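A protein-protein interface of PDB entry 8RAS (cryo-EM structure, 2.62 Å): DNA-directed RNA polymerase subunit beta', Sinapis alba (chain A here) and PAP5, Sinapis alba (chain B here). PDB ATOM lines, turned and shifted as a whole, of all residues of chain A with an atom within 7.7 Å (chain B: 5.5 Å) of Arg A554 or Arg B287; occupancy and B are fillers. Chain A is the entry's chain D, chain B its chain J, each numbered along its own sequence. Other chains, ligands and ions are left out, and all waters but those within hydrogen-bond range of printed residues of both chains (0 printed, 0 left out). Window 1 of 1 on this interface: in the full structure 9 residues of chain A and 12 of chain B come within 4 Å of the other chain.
Ile A550 touches Leu B290.
Ala A552 touches Leu B290.
Asn A553 touches Leu B290.
Arg A554 touches Gly B210 (O to O, 3.9 Å).
CG of Pro B212 touches NH2 of Arg A554, 3.8 Å away.
NH2 of Arg A554 touches CG1 of Val B269, at 3.8 Å.
N of Arg A554 touches CD1 of Leu B290, at 3.7 Å.
Arg A554 touches Phe B291 (NE to CE1, 3.6 Å).
Tyr A555 touches Leu B209 (CA to O, 3.4 Å).
Of the 16 printed residues of chain B, 10 touch a printed residue of chain A.
Hydrophobic or aromatic side chains of chain B within 4 Å of the printed part of chain A: Pro B212, Val B269, His B289, Leu B290 and Phe B291.
Printed residues of chain A that touch a printed residue of chain B: Ile A550, Cys A551, Ala A552, Asn A553, Arg A554, Tyr A555 and Asn A556.
Among the printed residues, 16 pairs touch across the chains.
The backbone carbonyl oxygen (O) of Ile A550 lies within hydrogen-bond range of the guanidinium group (NH1) of Arg B287 (2.7 Å).
A ring nitrogen (NE2) of His B289 lies within hydrogen-bond range of the backbone carbonyl oxygen of Cys A551.
The guanidinium group (NH1) of Arg B287 sits at hydrogen-bond distance from the backbone carbonyl oxygen (O) of Asn A553 (3.3 Å).
NH2 of Arg A554 is in hydrogen-bond range of O of Gln B268 (2.9 Å).
The guanidinium group (NH2) of Arg B287 sits at hydrogen-bond distance from the backbone carbonyl oxygen (O) of Arg A554 (2.9 Å).
OE1 of Glu B294 lies within salt-bridge range of NH1 of Arg A554, 3.2 Å away.
The backbone NH of Asn A556 is in hydrogen-bond range of the backbone carbonyl oxygen of Leu B209, 3.0 Å away.
OH of Tyr A555 lies close to NE of Arg A554, 3.5 Å away.
NE2 of Gln B268 is in hydrogen-bond range of O of Phe B291 (3.3 Å).
NE2 of Gln B268 is in hydrogen-bond range of OE1 of Glu B294 (3.0 Å).
Of chain B, only Gly B210 (3.9 Å), Pro B212 (3.8 Å), Gln B268 (2.9 Å), Val B269 (3.8 Å), Arg B287 (2.9 Å), Leu B290 (3.7 Å), Phe B291 (3.6 Å) and Glu B294 (3.1 Å) come within 4 Å of Arg A554.
Of chain A, only Ile A550 (2.7 Å), Asn A553 (3.3 Å) and Arg A554 (2.9 Å) come within 4 Å of Arg B287.
No residue of chain A comes within 4 Å of Ala B286.
Of the printed residues of chain A, Leu B290 touches Ile A550 (3.6 Å), Ala A552 (3.3 Å), Asn A553 (3.7 Å) and Arg A554 (3.7 Å).
Printed residues of chain A within 4 Å of Gly B210: Arg A554.
The nearest residue of chain B that does not touch Arg A554 is Leu B209 (4.8 Å).
The nearest printed residue of chain A that does not touch Gly B210 is Tyr A555 (4.1 Å).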
ATOM      1  N   GLY A 549      22.571   3.188   5.530  1.00  0.00           N
ATOM      2  CA  GLY A 549      23.617   2.741   6.432  1.00  0.00           C
ATOM      3  C   GLY A 549      23.534   1.256   6.714  1.00  0.00           C
ATOM      4  O   GLY A 549      23.382   0.434   5.806  1.00  0.00           O
ATOM      5  N   ILE A 550      23.644   0.903   7.997  1.00  0.00           N
ATOM      6  CA  ILE A 550      23.611  -0.496   8.405  1.00  0.00           C
ATOM      7  C   ILE A 550      22.249  -1.137   8.209  1.00  0.00           C
ATOM      8  O   ILE A 550      22.141  -2.365   8.264  1.00  0.00           O
ATOM      9  CB  ILE A 550      24.050  -0.634   9.877  1.00  0.00           C
ATOM     10  CG1 ILE A 550      23.119   0.161  10.791  1.00  0.00           C
ATOM     11  CG2 ILE A 550      25.484  -0.171  10.048  1.00  0.00           C
ATOM     12  CD1 ILE A 550      23.005  -0.409  12.178  1.00  0.00           C
ATOM     13  N   CYS A 551      21.208  -0.342   7.980  1.00  0.00           N
ATOM     14  CA  CYS A 551      19.884  -0.863   7.674  1.00  0.00           C
ATOM     15  C   CYS A 551      19.675  -1.094   6.183  1.00  0.00           C
ATOM     16  O   CYS A 551      18.592  -1.531   5.785  1.00  0.00           O
ATOM     17  CB  CYS A 551      18.806   0.087   8.203  1.00  0.00           C
ATOM     18  SG  CYS A 551      18.648   0.106  10.003  1.00  0.00           S
ATOM     19  N   ALA A 552      20.677  -0.814   5.359  1.00  0.00           N
ATOM     20  CA  ALA A 552      20.605  -1.024   3.920  1.00  0.00           C
ATOM     21  C   ALA A 552      21.603  -2.050   3.414  1.00  0.00           C
ATOM     22  O   ALA A 552      21.294  -2.791   2.479  1.00  0.00           O
ATOM     23  CB  ALA A 552      20.826   0.301   3.180  1.00  0.00           C
ATOM     24  N   ASN A 553      22.795  -2.108   4.001  1.00  0.00           N
ATOM     25  CA  ASN A 553      23.822  -3.056   3.600  1.00  0.00           C
ATOM     26  C   ASN A 553      24.265  -3.865   4.807  1.00  0.00           C
ATOM     27  O   ASN A 553      24.436  -3.319   5.900  1.00  0.00           O
ATOM     28  CB  ASN A 553      25.036  -2.349   2.982  1.00  0.00           C
ATOM     29  CG  ASN A 553      24.659  -1.424   1.847  1.00  0.00           C
ATOM     30  OD1 ASN A 553      24.200  -1.868   0.797  1.00  0.00           O
ATOM     31  ND2 ASN A 553      24.859  -0.129   2.050  1.00  0.00           N
ATOM     32  N   ARG A 554      24.446  -5.170   4.602  1.00  0.00           N
ATOM     33  CA  ARG A 554      24.971  -6.016   5.667  1.00  0.00           C
ATOM     34  C   ARG A 554      26.426  -5.696   5.971  1.00  0.00           C
ATOM     35  O   ARG A 554      26.846  -5.764   7.130  1.00  0.00           O
ATOM     36  CB  ARG A 554      24.822  -7.488   5.292  1.00  0.00           C
ATOM     37  CG  ARG A 554      24.713  -8.422   6.481  1.00  0.00           C
ATOM     38  CD  ARG A 554      25.264  -9.793   6.143  1.00  0.00           C
ATOM     39  NE  ARG A 554      25.918 -10.429   7.279  1.00  0.00           N
ATOM     40  CZ  ARG A 554      25.981 -11.740   7.464  1.00  0.00           C
ATOM     41  NH1 ARG A 554      25.427 -12.586   6.611  1.00  0.00           N
ATOM     42  NH2 ARG A 554      26.616 -12.215   8.531  1.00  0.00           N
ATOM     43  N   TYR A 555      27.203  -5.346   4.953  1.00  0.00           N
ATOM     44  CA  TYR A 555      28.622  -5.082   5.101  1.00  0.00           C
ATOM     45  C   TYR A 555      28.923  -3.636   4.737  1.00  0.00           C
ATOM     46  O   TYR A 555      28.164  -2.980   4.019  1.00  0.00           O
ATOM     47  CB  TYR A 555      29.453  -6.025   4.223  1.00  0.00           C
ATOM     48  CG  TYR A 555      29.252  -7.486   4.542  1.00  0.00           C
ATOM     49  CD1 TYR A 555      29.690  -8.021   5.746  1.00  0.00           C
ATOM     50  CD2 TYR A 555      28.613  -8.330   3.645  1.00  0.00           C
ATOM     51  CE1 TYR A 555      29.505  -9.355   6.042  1.00  0.00           C
ATOM     52  CE2 TYR A 555      28.422  -9.665   3.934  1.00  0.00           C
ATOM     53  CZ  TYR A 555      28.869 -10.172   5.132  1.00  0.00           C
ATOM     54  OH  TYR A 555      28.683 -11.503   5.422  1.00  0.00           O
ATOM     55  N   ASN A 556      30.041  -3.145   5.255  1.00  0.00           N
ATOM     56  CA  ASN A 556      30.508  -1.815   4.907  1.00  0.00           C
ATOM     57  C   ASN A 556      30.819  -1.760   3.414  1.00  0.00           C
ATOM     58  O   ASN A 556      31.606  -2.581   2.922  1.00  0.00           O
ATOM     59  CB  ASN A 556      31.755  -1.475   5.721  1.00  0.00           C
ATOM     60  CG  ASN A 556      32.069   0.004   5.738  1.00  0.00           C
ATOM     61  OD1 ASN A 556      31.383   0.808   5.111  1.00  0.00           O
ATOM     62  ND2 ASN A 556      33.118   0.373   6.460  1.00  0.00           N
ATOM     63  N   PRO A 557      30.232  -0.827   2.663  1.00  0.00           N
ATOM     64  CA  PRO A 557      30.547  -0.737   1.230  1.00  0.00           C
ATOM     65  C   PRO A 557      31.956  -0.223   0.986  1.00  0.00           C
ATOM     66  O   PRO A 557      32.139   0.859   0.422  1.00  0.00           O
ATOM     67  CB  PRO A 557      29.490   0.237   0.692  1.00  0.00           C
ATOM     68  CG  PRO A 557      28.464   0.363   1.774  1.00  0.00           C
ATOM     69  CD  PRO A 557      29.177   0.121   3.055  1.00  0.00           C
ATOM     70  N   LEU B 209      34.637  -4.142   8.291  1.00  0.00           N
ATOM     71  CA  LEU B 209      33.837  -4.730   7.225  1.00  0.00           C
ATOM     72  C   LEU B 209      32.397  -5.003   7.634  1.00  0.00           C
ATOM     73  O   LEU B 209      31.562  -5.248   6.759  1.00  0.00           O
ATOM     74  CB  LEU B 209      34.477  -6.035   6.745  1.00  0.00           C
ATOM     75  CG  LEU B 209      35.711  -5.922   5.852  1.00  0.00           C
ATOM     76  CD1 LEU B 209      36.101  -7.286   5.317  1.00  0.00           C
ATOM     77  CD2 LEU B 209      35.458  -4.954   4.713  1.00  0.00           C
ATOM     78  N   GLY B 210      32.085  -4.966   8.926  1.00  0.00           N
ATOM     79  CA  GLY B 210      30.761  -5.324   9.382  1.00  0.00           C
ATOM     80  C   GLY B 210      30.531  -6.805   9.559  1.00  0.00           C
ATOM     81  O   GLY B 210      29.385  -7.219   9.761  1.00  0.00           O
ATOM     82  N   PRO B 212      30.592 -10.461  11.508  1.00  0.00           N
ATOM     83  CA  PRO B 212      30.282 -10.758  12.913  1.00  0.00           C
ATOM     84  C   PRO B 212      31.528 -10.743  13.788  1.00  0.00           C
ATOM     85  O   PRO B 212      32.510 -11.437  13.518  1.00  0.00           O
ATOM     86  CB  PRO B 212      29.651 -12.150  12.845  1.00  0.00           C
ATOM     87  CG  PRO B 212      29.075 -12.228  11.485  1.00  0.00           C
ATOM     88  CD  PRO B 212      30.008 -11.459  10.597  1.00  0.00           C
ATOM     89  N   GLN B 268      25.039 -18.383   9.148  1.00  0.00           N
ATOM     90  CA  GLN B 268      24.870 -17.067   8.538  1.00  0.00           C
ATOM     91  C   GLN B 268      25.423 -15.972   9.440  1.00  0.00           C
ATOM     92  O   GLN B 268      26.082 -15.040   8.967  1.00  0.00           O
ATOM     93  CB  GLN B 268      23.394 -16.820   8.231  1.00  0.00           C
ATOM     94  CG  GLN B 268      23.130 -15.598   7.370  1.00  0.00           C
ATOM     95  CD  GLN B 268      21.704 -15.541   6.861  1.00  0.00           C
ATOM     96  OE1 GLN B 268      20.857 -16.334   7.266  1.00  0.00           O
ATOM     97  NE2 GLN B 268      21.432 -14.602   5.967  1.00  0.00           N
ATOM     98  N   VAL B 269      25.160 -16.067  10.743  1.00  0.00           N
ATOM     99  CA  VAL B 269      25.735 -15.174  11.736  1.00  0.00           C
ATOM    100  C   VAL B 269      26.294 -16.024  12.868  1.00  0.00           C
ATOM    101  O   VAL B 269      25.931 -17.189  13.040  1.00  0.00           O
ATOM    102  CB  VAL B 269      24.712 -14.155  12.286  1.00  0.00           C
ATOM    103  CG1 VAL B 269      24.146 -13.300  11.163  1.00  0.00           C
ATOM    104  CG2 VAL B 269      23.598 -14.869  13.031  1.00  0.00           C
ATOM    105  N   SER B 282      18.042  -7.047  19.734  1.00  0.00           N
ATOM    106  CA  SER B 282      17.719  -5.722  19.213  1.00  0.00           C
ATOM    107  C   SER B 282      18.419  -5.461  17.885  1.00  0.00           C
ATOM    108  O   SER B 282      17.819  -4.906  16.955  1.00  0.00           O
ATOM    109  CB  SER B 282      18.096  -4.652  20.236  1.00  0.00           C
ATOM    110  OG  SER B 282      17.162  -4.614  21.299  1.00  0.00           O
ATOM    111  N   LEU B 283      19.689  -5.855  17.776  1.00  0.00           N
ATOM    112  CA  LEU B 283      20.415  -5.668  16.524  1.00  0.00           C
ATOM    113  C   LEU B 283      19.784  -6.470  15.391  1.00  0.00           C
ATOM    114  O   LEU B 283      19.676  -5.983  14.258  1.00  0.00           O
ATOM    115  CB  LEU B 283      21.880  -6.053  16.709  1.00  0.00           C
ATOM    116  CG  LEU B 283      22.803  -5.762  15.529  1.00  0.00           C
ATOM    117  CD1 LEU B 283      22.763  -4.286  15.181  1.00  0.00           C
ATOM    118  CD2 LEU B 283      24.215  -6.206  15.852  1.00  0.00           C
ATOM    119  N   TYR B 284      19.370  -7.707  15.672  1.00  0.00           N
ATOM    120  CA  TYR B 284      18.680  -8.497  14.658  1.00  0.00           C
ATOM    121  C   TYR B 284      17.354  -7.861  14.272  1.00  0.00           C
ATOM    122  O   TYR B 284      16.984  -7.850  13.095  1.00  0.00           O
ATOM    123  CB  TYR B 284      18.456  -9.927  15.148  1.00  0.00           C
ATOM    124  CG  TYR B 284      17.503 -10.705  14.268  1.00  0.00           C
ATOM    125  CD1 TYR B 284      17.943 -11.300  13.096  1.00  0.00           C
ATOM    126  CD2 TYR B 284      16.163 -10.834  14.605  1.00  0.00           C
ATOM    127  CE1 TYR B 284      17.078 -12.001  12.285  1.00  0.00           C
ATOM    128  CE2 TYR B 284      15.291 -11.532  13.801  1.00  0.00           C
ATOM    129  CZ  TYR B 284      15.754 -12.114  12.643  1.00  0.00           C
ATOM    130  OH  TYR B 284      14.886 -12.813  11.839  1.00  0.00           O
ATOM    131  N   ARG B 285      16.609  -7.347  15.252  1.00  0.00           N
ATOM    132  CA  ARG B 285      15.369  -6.653  14.934  1.00  0.00           C
ATOM    133  C   ARG B 285      15.626  -5.456  14.032  1.00  0.00           C
ATOM    134  O   ARG B 285      14.796  -5.129  13.177  1.00  0.00           O
ATOM    135  CB  ARG B 285      14.676  -6.217  16.223  1.00  0.00           C
ATOM    136  CG  ARG B 285      13.294  -5.640  16.030  1.00  0.00           C
ATOM    137  CD  ARG B 285      12.606  -5.445  17.365  1.00  0.00           C
ATOM    138  NE  ARG B 285      13.398  -4.621  18.270  1.00  0.00           N
ATOM    139  CZ  ARG B 285      13.947  -5.057  19.396  1.00  0.00           C
ATOM    140  NH1 ARG B 285      13.813  -6.312  19.790  1.00  0.00           N
ATOM    141  NH2 ARG B 285      14.650  -4.212  20.144  1.00  0.00           N
ATOM    142  N   ALA B 286      16.771  -4.796  14.208  1.00  0.00           N
ATOM    143  CA  ALA B 286      17.111  -3.667  13.348  1.00  0.00           C
ATOM    144  C   ALA B 286      17.477  -4.118  11.937  1.00  0.00           C
ATOM    145  O   ALA B 286      17.087  -3.476  10.957  1.00  0.00           O
ATOM    146  CB  ALA B 286      18.255  -2.867  13.966  1.00  0.00           C
ATOM    147  N   ARG B 287      18.227  -5.214  11.811  1.00  0.00           N
ATOM    148  CA  ARG B 287      18.839  -5.587  10.539  1.00  0.00           C
ATOM    149  C   ARG B 287      18.274  -6.875   9.942  1.00  0.00           C
ATOM    150  O   ARG B 287      18.948  -7.520   9.134  1.00  0.00           O
ATOM    151  CB  ARG B 287      20.352  -5.720  10.711  1.00  0.00           C
ATOM    152  CG  ARG B 287      21.100  -4.405  10.703  1.00  0.00           C
ATOM    153  CD  ARG B 287      22.451  -4.543  11.374  1.00  0.00           C
ATOM    154  NE  ARG B 287      23.296  -5.530  10.715  1.00  0.00           N
ATOM    155  CZ  ARG B 287      24.032  -5.292   9.639  1.00  0.00           C
ATOM    156  NH1 ARG B 287      24.043  -4.106   9.058  1.00  0.00           N
ATOM    157  NH2 ARG B 287      24.780  -6.269   9.136  1.00  0.00           N
ATOM    158  N   ARG B 288      17.049  -7.256  10.302  1.00  0.00           N
ATOM    159  CA  ARG B 288      16.556  -8.589   9.967  1.00  0.00           C
ATOM    160  C   ARG B 288      16.164  -8.754   8.504  1.00  0.00           C
ATOM    161  O   ARG B 288      16.088  -9.891   8.029  1.00  0.00           O
ATOM    162  CB  ARG B 288      15.366  -8.947  10.862  1.00  0.00           C
ATOM    163  CG  ARG B 288      14.106  -8.152  10.593  1.00  0.00           C
ATOM    164  CD  ARG B 288      13.072  -8.389  11.678  1.00  0.00           C
ATOM    165  NE  ARG B 288      11.766  -7.853  11.315  1.00  0.00           N
ATOM    166  CZ  ARG B 288      11.270  -6.711  11.768  1.00  0.00           C
ATOM    167  NH1 ARG B 288      11.943  -5.951  12.616  1.00  0.00           N
ATOM    168  NH2 ARG B 288      10.065  -6.320  11.362  1.00  0.00           N
ATOM    169  N   HIS B 289      15.914  -7.662   7.780  1.00  0.00           N
ATOM    170  CA  HIS B 289      15.485  -7.788   6.389  1.00  0.00           C
ATOM    171  C   HIS B 289      16.628  -8.213   5.475  1.00  0.00           C
ATOM    172  O   HIS B 289      16.399  -8.917   4.483  1.00  0.00           O
ATOM    173  CB  HIS B 289      14.877  -6.469   5.910  1.00  0.00           C
ATOM    174  CG  HIS B 289      15.730  -5.273   6.191  1.00  0.00           C
ATOM    175  ND1 HIS B 289      15.800  -4.681   7.434  1.00  0.00           N
ATOM    176  CD2 HIS B 289      16.553  -4.557   5.388  1.00  0.00           C
ATOM    177  CE1 HIS B 289      16.628  -3.653   7.384  1.00  0.00           C
ATOM    178  NE2 HIS B 289      17.097  -3.556   6.154  1.00  0.00           N
ATOM    179  N   LEU B 290      17.858  -7.804   5.792  1.00  0.00           N
ATOM    180  CA  LEU B 290      19.001  -8.141   4.950  1.00  0.00           C
ATOM    181  C   LEU B 290      19.254  -9.645   4.927  1.00  0.00           C
ATOM    182  O   LEU B 290      19.543 -10.220   3.871  1.00  0.00           O
ATOM    183  CB  LEU B 290      20.241  -7.394   5.439  1.00  0.00           C
ATOM    184  CG  LEU B 290      20.073  -5.890   5.670  1.00  0.00           C
ATOM    185  CD1 LEU B 290      21.240  -5.329   6.462  1.00  0.00           C
ATOM    186  CD2 LEU B 290      19.921  -5.158   4.352  1.00  0.00           C
ATOM    187  N   PHE B 291      19.145 -10.299   6.084  1.00  0.00           N
ATOM    188  CA  PHE B 291      19.396 -11.735   6.149  1.00  0.00           C
ATOM    189  C   PHE B 291      18.317 -12.521   5.412  1.00  0.00           C
ATOM    190  O   PHE B 291      18.615 -13.509   4.727  1.00  0.00           O
ATOM    191  CB  PHE B 291      19.495 -12.169   7.610  1.00  0.00           C
ATOM    192  CG  PHE B 291      20.442 -11.335   8.420  1.00  0.00           C
ATOM    193  CD1 PHE B 291      21.798 -11.335   8.141  1.00  0.00           C
ATOM    194  CD2 PHE B 291      19.979 -10.545   9.456  1.00  0.00           C
ATOM    195  CE1 PHE B 291      22.671 -10.564   8.882  1.00  0.00           C
ATOM    196  CE2 PHE B 291      20.849  -9.774  10.201  1.00  0.00           C
ATOM    197  CZ  PHE B 291      22.197  -9.784   9.911  1.00  0.00           C
ATOM    198  N   GLU B 294      19.097 -12.246   1.809  1.00  0.00           N
ATOM    199  CA  GLU B 294      20.172 -13.168   1.452  1.00  0.00           C
ATOM    200  C   GLU B 294      19.651 -14.589   1.286  1.00  0.00           C
ATOM    201  O   GLU B 294      20.035 -15.295   0.344  1.00  0.00           O
ATOM    202  CB  GLU B 294      21.276 -13.130   2.504  1.00  0.00           C
ATOM    203  CG  GLU B 294      22.072 -11.851   2.520  1.00  0.00           C
ATOM    204  CD  GLU B 294      23.181 -11.879   3.546  1.00  0.00           C
ATOM    205  OE1 GLU B 294      23.175 -12.787   4.401  1.00  0.00           O
ATOM    206  OE2 GLU B 294      24.062 -10.997   3.492  1.00  0.00           O
